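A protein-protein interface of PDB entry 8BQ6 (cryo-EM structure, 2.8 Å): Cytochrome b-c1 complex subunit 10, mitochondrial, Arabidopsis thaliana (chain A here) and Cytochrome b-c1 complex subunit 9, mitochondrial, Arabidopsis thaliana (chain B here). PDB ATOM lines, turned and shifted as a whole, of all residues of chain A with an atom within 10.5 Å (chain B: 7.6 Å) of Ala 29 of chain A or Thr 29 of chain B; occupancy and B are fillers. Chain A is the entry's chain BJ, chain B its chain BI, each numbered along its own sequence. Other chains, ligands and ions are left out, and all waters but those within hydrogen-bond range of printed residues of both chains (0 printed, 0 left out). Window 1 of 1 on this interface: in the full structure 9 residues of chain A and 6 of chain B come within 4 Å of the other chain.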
ATOM      1  N   GLN A  21       3.894 -15.068  -7.354  1.00  0.00           N
ATOM      2  CA  GLN A  21       3.098 -14.757  -6.174  1.00  0.00           C
ATOM      3  C   GLN A  21       2.855 -16.006  -5.339  1.00  0.00           C
ATOM      4  O   GLN A  21       3.028 -15.986  -4.115  1.00  0.00           O
ATOM      5  CB  GLN A  21       1.774 -14.114  -6.589  1.00  0.00           C
ATOM      6  CG  GLN A  21       1.097 -13.268  -5.510  1.00  0.00           C
ATOM      7  CD  GLN A  21       0.575 -14.077  -4.332  1.00  0.00           C
ATOM      8  OE1 GLN A  21       0.103 -15.204  -4.493  1.00  0.00           O
ATOM      9  NE2 GLN A  21       0.650 -13.497  -3.141  1.00  0.00           N
ATOM     10  N   ALA A  22       2.470 -17.110  -5.983  1.00  0.00           N
ATOM     11  CA  ALA A  22       2.248 -18.343  -5.238  1.00  0.00           C
ATOM     12  C   ALA A  22       3.545 -18.856  -4.626  1.00  0.00           C
ATOM     13  O   ALA A  22       3.542 -19.415  -3.524  1.00  0.00           O
ATOM     14  CB  ALA A  22       1.619 -19.404  -6.141  1.00  0.00           C
ATOM     15  N   ALA A  23       4.667 -18.670  -5.327  1.00  0.00           N
ATOM     16  CA  ALA A  23       5.956 -19.106  -4.801  1.00  0.00           C
ATOM     17  C   ALA A  23       6.363 -18.306  -3.569  1.00  0.00           C
ATOM     18  O   ALA A  23       6.903 -18.865  -2.608  1.00  0.00           O
ATOM     19  CB  ALA A  23       7.027 -18.995  -5.883  1.00  0.00           C
ATOM     20  N   ALA A  24       6.141 -16.989  -3.590  1.00  0.00           N
ATOM     21  CA  ALA A  24       6.436 -16.177  -2.414  1.00  0.00           C
ATOM     22  C   ALA A  24       5.469 -16.487  -1.280  1.00  0.00           C
ATOM     23  O   ALA A  24       5.848 -16.454  -0.103  1.00  0.00           O
ATOM     24  CB  ALA A  24       6.385 -14.691  -2.768  1.00  0.00           C
ATOM     25  N   GLY A  25       4.212 -16.781  -1.616  1.00  0.00           N
ATOM     26  CA  GLY A  25       3.235 -17.097  -0.587  1.00  0.00           C
ATOM     27  C   GLY A  25       3.544 -18.390   0.141  1.00  0.00           C
ATOM     28  O   GLY A  25       3.427 -18.466   1.366  1.00  0.00           O
ATOM     29  N   TRP A  26       3.935 -19.429  -0.600  1.00  0.00           N
ATOM     30  CA  TRP A  26       4.308 -20.679   0.048  1.00  0.00           C
ATOM     31  C   TRP A  26       5.648 -20.555   0.757  1.00  0.00           C
ATOM     32  O   TRP A  26       5.850 -21.167   1.811  1.00  0.00           O
ATOM     33  CB  TRP A  26       4.338 -21.813  -0.974  1.00  0.00           C
ATOM     34  CG  TRP A  26       2.975 -22.284  -1.349  1.00  0.00           C
ATOM     35  CD1 TRP A  26       2.407 -22.233  -2.586  1.00  0.00           C
ATOM     36  CD2 TRP A  26       2.001 -22.879  -0.482  1.00  0.00           C
ATOM     37  NE1 TRP A  26       1.137 -22.755  -2.544  1.00  0.00           N
ATOM     38  CE2 TRP A  26       0.866 -23.161  -1.264  1.00  0.00           C
ATOM     39  CE3 TRP A  26       1.981 -23.203   0.878  1.00  0.00           C
ATOM     40  CZ2 TRP A  26      -0.279 -23.747  -0.733  1.00  0.00           C
ATOM     41  CZ3 TRP A  26       0.844 -23.784   1.403  1.00  0.00           C
ATOM     42  CH2 TRP A  26      -0.270 -24.051   0.599  1.00  0.00           C
ATOM     43  N   GLY A  27       6.568 -19.767   0.198  1.00  0.00           N
ATOM     44  CA  GLY A  27       7.813 -19.494   0.895  1.00  0.00           C
ATOM     45  C   GLY A  27       7.594 -18.778   2.213  1.00  0.00           C
ATOM     46  O   GLY A  27       8.345 -18.976   3.171  1.00  0.00           O
ATOM     47  N   ILE A  28       6.573 -17.919   2.277  1.00  0.00           N
ATOM     48  CA  ILE A  28       6.215 -17.289   3.545  1.00  0.00           C
ATOM     49  C   ILE A  28       5.597 -18.310   4.487  1.00  0.00           C
ATOM     50  O   ILE A  28       5.901 -18.338   5.686  1.00  0.00           O
ATOM     51  CB  ILE A  28       5.267 -16.100   3.308  1.00  0.00           C
ATOM     52  CG1 ILE A  28       6.048 -14.900   2.783  1.00  0.00           C
ATOM     53  CG2 ILE A  28       4.540 -15.738   4.598  1.00  0.00           C
ATOM     54  CD1 ILE A  28       5.302 -13.606   2.899  1.00  0.00           C
ATOM     55  N   ALA A  29       4.717 -19.164   3.958  1.00  0.00           N
ATOM     56  CA  ALA A  29       4.085 -20.189   4.779  1.00  0.00           C
ATOM     57  C   ALA A  29       5.120 -21.141   5.360  1.00  0.00           C
ATOM     58  O   ALA A  29       5.024 -21.541   6.527  1.00  0.00           O
ATOM     59  CB  ALA A  29       3.054 -20.958   3.954  1.00  0.00           C
ATOM     60  N   ALA A  30       6.119 -21.517   4.559  1.00  0.00           N
ATOM     61  CA  ALA A  30       7.163 -22.417   5.036  1.00  0.00           C
ATOM     62  C   ALA A  30       8.025 -21.755   6.104  1.00  0.00           C
ATOM     63  O   ALA A  30       8.433 -22.403   7.074  1.00  0.00           O
ATOM     64  CB  ALA A  30       8.023 -22.881   3.864  1.00  0.00           C
ATOM     65  N   ALA A  31       8.331 -20.467   5.930  1.00  0.00           N
ATOM     66  CA  ALA A  31       9.158 -19.763   6.905  1.00  0.00           C
ATOM     67  C   ALA A  31       8.417 -19.575   8.220  1.00  0.00           C
ATOM     68  O   ALA A  31       8.996 -19.751   9.298  1.00  0.00           O
ATOM     69  CB  ALA A  31       9.602 -18.416   6.339  1.00  0.00           C
ATOM     70  N   ALA A  32       7.135 -19.212   8.151  1.00  0.00           N
ATOM     71  CA  ALA A  32       6.328 -19.126   9.362  1.00  0.00           C
ATOM     72  C   ALA A  32       6.223 -20.481  10.046  1.00  0.00           C
ATOM     73  O   ALA A  32       6.264 -20.568  11.279  1.00  0.00           O
ATOM     74  CB  ALA A  32       4.938 -18.584   9.032  1.00  0.00           C
ATOM     75  N   GLY A  33       6.080 -21.552   9.261  1.00  0.00           N
ATOM     76  CA  GLY A  33       6.005 -22.881   9.845  1.00  0.00           C
ATOM     77  C   GLY A  33       7.292 -23.297  10.529  1.00  0.00           C
ATOM     78  O   GLY A  33       7.266 -23.946  11.579  1.00  0.00           O
ATOM     79  N   ALA A  34       8.437 -22.941   9.939  1.00  0.00           N
ATOM     80  CA  ALA A  34       9.719 -23.201  10.586  1.00  0.00           C
ATOM     81  C   ALA A  34       9.840 -22.436  11.897  1.00  0.00           C
ATOM     82  O   ALA A  34      10.316 -22.981  12.899  1.00  0.00           O
ATOM     83  CB  ALA A  34      10.866 -22.835   9.646  1.00  0.00           C
ATOM     84  N   ILE A  35       9.417 -21.171  11.907  1.00  0.00           N
ATOM     85  CA  ILE A  35       9.415 -20.399  13.143  1.00  0.00           C
ATOM     86  C   ILE A  35       8.409 -20.971  14.139  1.00  0.00           C
ATOM     87  O   ILE A  35       8.559 -20.796  15.355  1.00  0.00           O
ATOM     88  CB  ILE A  35       9.147 -18.915  12.824  1.00  0.00           C
ATOM     89  CG1 ILE A  35      10.295 -18.343  11.990  1.00  0.00           C
ATOM     90  CG2 ILE A  35       8.976 -18.094  14.089  1.00  0.00           C
ATOM     91  CD1 ILE A  35       9.892 -17.214  11.073  1.00  0.00           C
ATOM     92  N   TRP A  36       7.387 -21.678  13.657  1.00  0.00           N
ATOM     93  CA  TRP A  36       6.355 -22.196  14.550  1.00  0.00           C
ATOM     94  C   TRP A  36       6.750 -23.538  15.158  1.00  0.00           C
ATOM     95  O   TRP A  36       6.553 -23.758  16.358  1.00  0.00           O
ATOM     96  CB  TRP A  36       5.035 -22.321  13.794  1.00  0.00           C
ATOM     97  CG  TRP A  36       3.974 -23.099  14.506  1.00  0.00           C
ATOM     98  CD1 TRP A  36       3.381 -22.782  15.690  1.00  0.00           C
ATOM     99  CD2 TRP A  36       3.362 -24.315  14.064  1.00  0.00           C
ATOM    100  NE1 TRP A  36       2.444 -23.730  16.019  1.00  0.00           N
ATOM    101  CE2 TRP A  36       2.412 -24.681  15.034  1.00  0.00           C
ATOM    102  CE3 TRP A  36       3.530 -25.132  12.943  1.00  0.00           C
ATOM    103  CZ2 TRP A  36       1.634 -25.829  14.920  1.00  0.00           C
ATOM    104  CZ3 TRP A  36       2.757 -26.270  12.831  1.00  0.00           C
ATOM    105  CH2 TRP A  36       1.821 -26.607  13.812  1.00  0.00           C
ATOM    106  N   VAL A  37       7.293 -24.446  14.346  1.00  0.00           N
ATOM    107  CA  VAL A  37       7.746 -25.735  14.861  1.00  0.00           C
ATOM    108  C   VAL A  37       8.994 -25.554  15.714  1.00  0.00           C
ATOM    109  O   VAL A  37       9.009 -25.876  16.907  1.00  0.00           O
ATOM    110  CB  VAL A  37       7.985 -26.720  13.704  1.00  0.00           C
ATOM    111  CG1 VAL A  37       8.930 -27.824  14.129  1.00  0.00           C
ATOM    112  CG2 VAL A  37       6.667 -27.310  13.251  1.00  0.00           C
ATOM    113  N   ILE B  20      -6.904 -14.004   2.728  1.00  0.00           N
ATOM    114  CA  ILE B  20      -7.049 -15.283   3.413  1.00  0.00           C
ATOM    115  C   ILE B  20      -7.954 -16.222   2.629  1.00  0.00           C
ATOM    116  O   ILE B  20      -7.626 -17.397   2.437  1.00  0.00           O
ATOM    117  CB  ILE B  20      -7.562 -15.071   4.847  1.00  0.00           C
ATOM    118  CG1 ILE B  20      -6.533 -14.296   5.661  1.00  0.00           C
ATOM    119  CG2 ILE B  20      -7.838 -16.406   5.522  1.00  0.00           C
ATOM    120  CD1 ILE B  20      -7.075 -13.750   6.956  1.00  0.00           C
ATOM    121  N   ARG B  23      -6.338 -17.059  -1.340  1.00  0.00           N
ATOM    122  CA  ARG B  23      -5.091 -17.779  -1.552  1.00  0.00           C
ATOM    123  C   ARG B  23      -4.881 -18.756  -0.406  1.00  0.00           C
ATOM    124  O   ARG B  23      -4.887 -18.357   0.763  1.00  0.00           O
ATOM    125  CB  ARG B  23      -3.910 -16.813  -1.659  1.00  0.00           C
ATOM    126  CG  ARG B  23      -3.842 -16.049  -2.970  1.00  0.00           C
ATOM    127  CD  ARG B  23      -3.450 -16.961  -4.120  1.00  0.00           C
ATOM    128  NE  ARG B  23      -3.575 -16.302  -5.414  1.00  0.00           N
ATOM    129  CZ  ARG B  23      -4.677 -16.302  -6.150  1.00  0.00           C
ATOM    130  NH1 ARG B  23      -5.777 -16.918  -5.749  1.00  0.00           N
ATOM    131  NH2 ARG B  23      -4.678 -15.666  -7.317  1.00  0.00           N
ATOM    132  N   ASN B  24      -4.697 -20.031  -0.746  1.00  0.00           N
ATOM    133  CA  ASN B  24      -4.522 -21.054   0.278  1.00  0.00           C
ATOM    134  C   ASN B  24      -3.194 -20.912   1.009  1.00  0.00           C
ATOM    135  O   ASN B  24      -3.069 -21.363   2.152  1.00  0.00           O
ATOM    136  CB  ASN B  24      -4.632 -22.441  -0.347  1.00  0.00           C
ATOM    137  CG  ASN B  24      -4.846 -23.525   0.681  1.00  0.00           C
ATOM    138  OD1 ASN B  24      -5.659 -23.382   1.590  1.00  0.00           O
ATOM    139  ND2 ASN B  24      -4.112 -24.620   0.545  1.00  0.00           N
ATOM    140  N   SER B  25      -2.187 -20.311   0.372  1.00  0.00           N
ATOM    141  CA  SER B  25      -0.919 -20.101   1.061  1.00  0.00           C
ATOM    142  C   SER B  25      -1.074 -19.106   2.203  1.00  0.00           C
ATOM    143  O   SER B  25      -0.465 -19.268   3.266  1.00  0.00           O
ATOM    144  CB  SER B  25       0.154 -19.638   0.077  1.00  0.00           C
ATOM    145  OG  SER B  25      -0.239 -18.459  -0.599  1.00  0.00           O
ATOM    146  N   VAL B  26      -1.879 -18.062   2.002  1.00  0.00           N
ATOM    147  CA  VAL B  26      -2.140 -17.110   3.075  1.00  0.00           C
ATOM    148  C   VAL B  26      -2.986 -17.759   4.165  1.00  0.00           C
ATOM    149  O   VAL B  26      -2.787 -17.512   5.360  1.00  0.00           O
ATOM    150  CB  VAL B  26      -2.806 -15.844   2.511  1.00  0.00           C
ATOM    151  CG1 VAL B  26      -3.205 -14.904   3.631  1.00  0.00           C
ATOM    152  CG2 VAL B  26      -1.867 -15.153   1.536  1.00  0.00           C
ATOM    153  N   TYR B  27      -3.942 -18.600   3.768  1.00  0.00           N
ATOM    154  CA  TYR B  27      -4.786 -19.287   4.741  1.00  0.00           C
ATOM    155  C   TYR B  27      -3.976 -20.251   5.599  1.00  0.00           C
ATOM    156  O   TYR B  27      -4.200 -20.357   6.809  1.00  0.00           O
ATOM    157  CB  TYR B  27      -5.912 -20.020   4.015  1.00  0.00           C
ATOM    158  CG  TYR B  27      -6.891 -20.712   4.927  1.00  0.00           C
ATOM    159  CD1 TYR B  27      -7.854 -19.991   5.614  1.00  0.00           C
ATOM    160  CD2 TYR B  27      -6.860 -22.087   5.088  1.00  0.00           C
ATOM    161  CE1 TYR B  27      -8.753 -20.620   6.446  1.00  0.00           C
ATOM    162  CE2 TYR B  27      -7.755 -22.725   5.916  1.00  0.00           C
ATOM    163  CZ  TYR B  27      -8.701 -21.986   6.592  1.00  0.00           C
ATOM    164  OH  TYR B  27      -9.596 -22.619   7.419  1.00  0.00           O
ATOM    165  N   VAL B  28      -3.033 -20.969   4.984  1.00  0.00           N
ATOM    166  CA  VAL B  28      -2.172 -21.876   5.737  1.00  0.00           C
ATOM    167  C   VAL B  28      -1.281 -21.096   6.697  1.00  0.00           C
ATOM    168  O   VAL B  28      -1.052 -21.519   7.837  1.00  0.00           O
ATOM    169  CB  VAL B  28      -1.354 -22.749   4.768  1.00  0.00           C
ATOM    170  CG1 VAL B  28      -0.189 -23.412   5.482  1.00  0.00           C
ATOM    171  CG2 VAL B  28      -2.246 -23.800   4.138  1.00  0.00           C
ATOM    172  N   THR B  29      -0.766 -19.945   6.256  1.00  0.00           N
ATOM    173  CA  THR B  29      -0.036 -19.063   7.161  1.00  0.00           C
ATOM    174  C   THR B  29      -0.933 -18.587   8.296  1.00  0.00           C
ATOM    175  O   THR B  29      -0.500 -18.505   9.452  1.00  0.00           O
ATOM    176  CB  THR B  29       0.523 -17.866   6.394  1.00  0.00           C
ATOM    177  OG1 THR B  29       1.272 -18.329   5.264  1.00  0.00           O
ATOM    178  CG2 THR B  29       1.426 -17.034   7.285  1.00  0.00           C
ATOM    179  N   PHE B  30      -2.187 -18.269   7.980  1.00  0.00           N
ATOM    180  CA  PHE B  30      -3.134 -17.849   9.005  1.00  0.00           C
ATOM    181  C   PHE B  30      -3.381 -18.964  10.016  1.00  0.00           C
ATOM    182  O   PHE B  30      -3.471 -18.707  11.222  1.00  0.00           O
ATOM    183  CB  PHE B  30      -4.431 -17.396   8.331  1.00  0.00           C
ATOM    184  CG  PHE B  30      -5.605 -17.291   9.256  1.00  0.00           C
ATOM    185  CD1 PHE B  30      -5.682 -16.270  10.183  1.00  0.00           C
ATOM    186  CD2 PHE B  30      -6.653 -18.188   9.164  1.00  0.00           C
ATOM    187  CE1 PHE B  30      -6.768 -16.164  11.023  1.00  0.00           C
ATOM    188  CE2 PHE B  30      -7.743 -18.085  10.003  1.00  0.00           C
ATOM    189  CZ  PHE B  30      -7.800 -17.071  10.933  1.00  0.00           C
ATOM    190  N   ILE B  31      -3.478 -20.210   9.546  1.00  0.00           N
ATOM    191  CA  ILE B  31      -3.675 -21.344  10.447  1.00  0.00           C
ATOM    192  C   ILE B  31      -2.479 -21.506  11.377  1.00  0.00           C
ATOM    193  O   ILE B  31      -2.633 -21.739  12.583  1.00  0.00           O
ATOM    194  CB  ILE B  31      -3.935 -22.629   9.639  1.00  0.00           C
ATOM    195  CG1 ILE B  31      -5.296 -22.563   8.945  1.00  0.00           C
ATOM    196  CG2 ILE B  31      -3.836 -23.861  10.532  1.00  0.00           C
ATOM    197  CD1 ILE B  31      -6.438 -22.243   9.863  1.00  0.00           C
ATOM    198  N   ILE B  32      -1.267 -21.396  10.829  1.00  0.00           N
ATOM    199  CA  ILE B  32      -0.058 -21.550  11.632  1.00  0.00           C
ATOM    200  C   ILE B  32       0.027 -20.454  12.687  1.00  0.00           C
ATOM    201  O   ILE B  32       0.378 -20.707  13.845  1.00  0.00           O
ATOM    202  CB  ILE B  32       1.184 -21.548  10.723  1.00  0.00           C
ATOM    203  CG1 ILE B  32       1.227 -22.815   9.874  1.00  0.00           C
ATOM    204  CG2 ILE B  32       2.449 -21.411  11.539  1.00  0.00           C
ATOM    205  CD1 ILE B  32       2.135 -22.694   8.683  1.00  0.00           C
ATOM    206  N   ALA B  33      -0.268 -19.215  12.293  1.00  0.00           N
ATOM    207  CA  ALA B  33      -0.226 -18.109  13.242  1.00  0.00           C
ATOM    208  C   ALA B  33      -1.292 -18.265  14.319  1.00  0.00           C
ATOM    209  O   ALA B  33      -1.036 -18.000  15.498  1.00  0.00           O
ATOM    210  CB  ALA B  33      -0.389 -16.779  12.507  1.00  0.00           C
ATOM    211  N   GLY B  34      -2.496 -18.687  13.931  1.00  0.00           N
ATOM    212  CA  GLY B  34      -3.549 -18.895  14.913  1.00  0.00           C
ATOM    213  C   GLY B  34      -3.258 -20.051  15.851  1.00  0.00           C
ATOM    214  O   GLY B  34      -3.625 -20.016  17.028  1.00  0.00           O
ATOM    215  N   ALA B  35      -2.622 -21.104  15.333  1.00  0.00           N
ATOM    216  CA  ALA B  35      -2.205 -22.212  16.186  1.00  0.00           C
ATOM    217  C   ALA B  35      -1.150 -21.757  17.183  1.00  0.00           C
ATOM    218  O   ALA B  35      -1.196 -22.119  18.364  1.00  0.00           O
ATOM    219  CB  ALA B  35      -1.673 -23.363  15.333  1.00  0.00           C
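Of chain B, only Ser 25 (3.96 Å), Thr 29 (3.4 Å) and Ile 32 (3.8 Å) come within 4 Å of Ala 29 of chain A. Of the printed residues of chain A, Thr 29 of chain B touches Ala 29. No residue of chain A comes within 4 Å of Val 26 of chain B. Ile 32 of chain B touches three residues of chain A. No residue of chain A comes within 4 Å of Ala 33 of chain B. Of the printed residues of chain B, Gly 25 of chain A touches Ser 25. Of the printed residues of chain B, Ala 32 of chain A touches Ile 32. Printed residues of chain B within 4 Å of Trp 36 of chain A: Ile 32. Of the printed residues of chain B, Gln 21 of chain A touches Arg 23 (3.9 Å). Ala 35 of chain B touches none of the printed residues of chain A. Ile 28 of chain A touches none of the printed residues of chain B. The nearest printed residue of chain B that does not touch Ala 32 of chain A is Thr 29 of chain B (4.2 Å).
O of Ser 25 of chain B lies within hydrogen-bond range of OG1 of Thr 29 of chain B (2.8 Å).
Of the 17 printed residues of chain A, 6 touch a printed residue of chain B. Hydrophobic or aromatic side chains of chain A that line the printed part of chain B: Trp 26, Ala 29 and Trp 36. Of the 14 printed residues of chain B, 5 touch a printed residue of chain A. Printed residues of chain B that touch a printed residue of chain A: Arg 23, Asn 24, Ser 25, Thr 29 and Ile 32. Among the printed residues, 9 pairs touch across the chains.
Among the printed residues, merely in contact across the chains: Gln 21 of chain A with Arg 23 of chain B, Gly 25 of chain A with Ser 25 of chain B, Trp 26 of chain A with Asn 24 of chain B, Trp 26 of chain A with Ser 25 of chain B, Ala 29 of chain A with Ser 25 of chain B, Ala 29 of chain A with Thr 29 of chain B, Ala 29 of chain A with Ile 32 of chain B, Ala 32 of chain A with Ile 32 of chain B and Trp 36 of chain A with Ile 32 of chain B.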
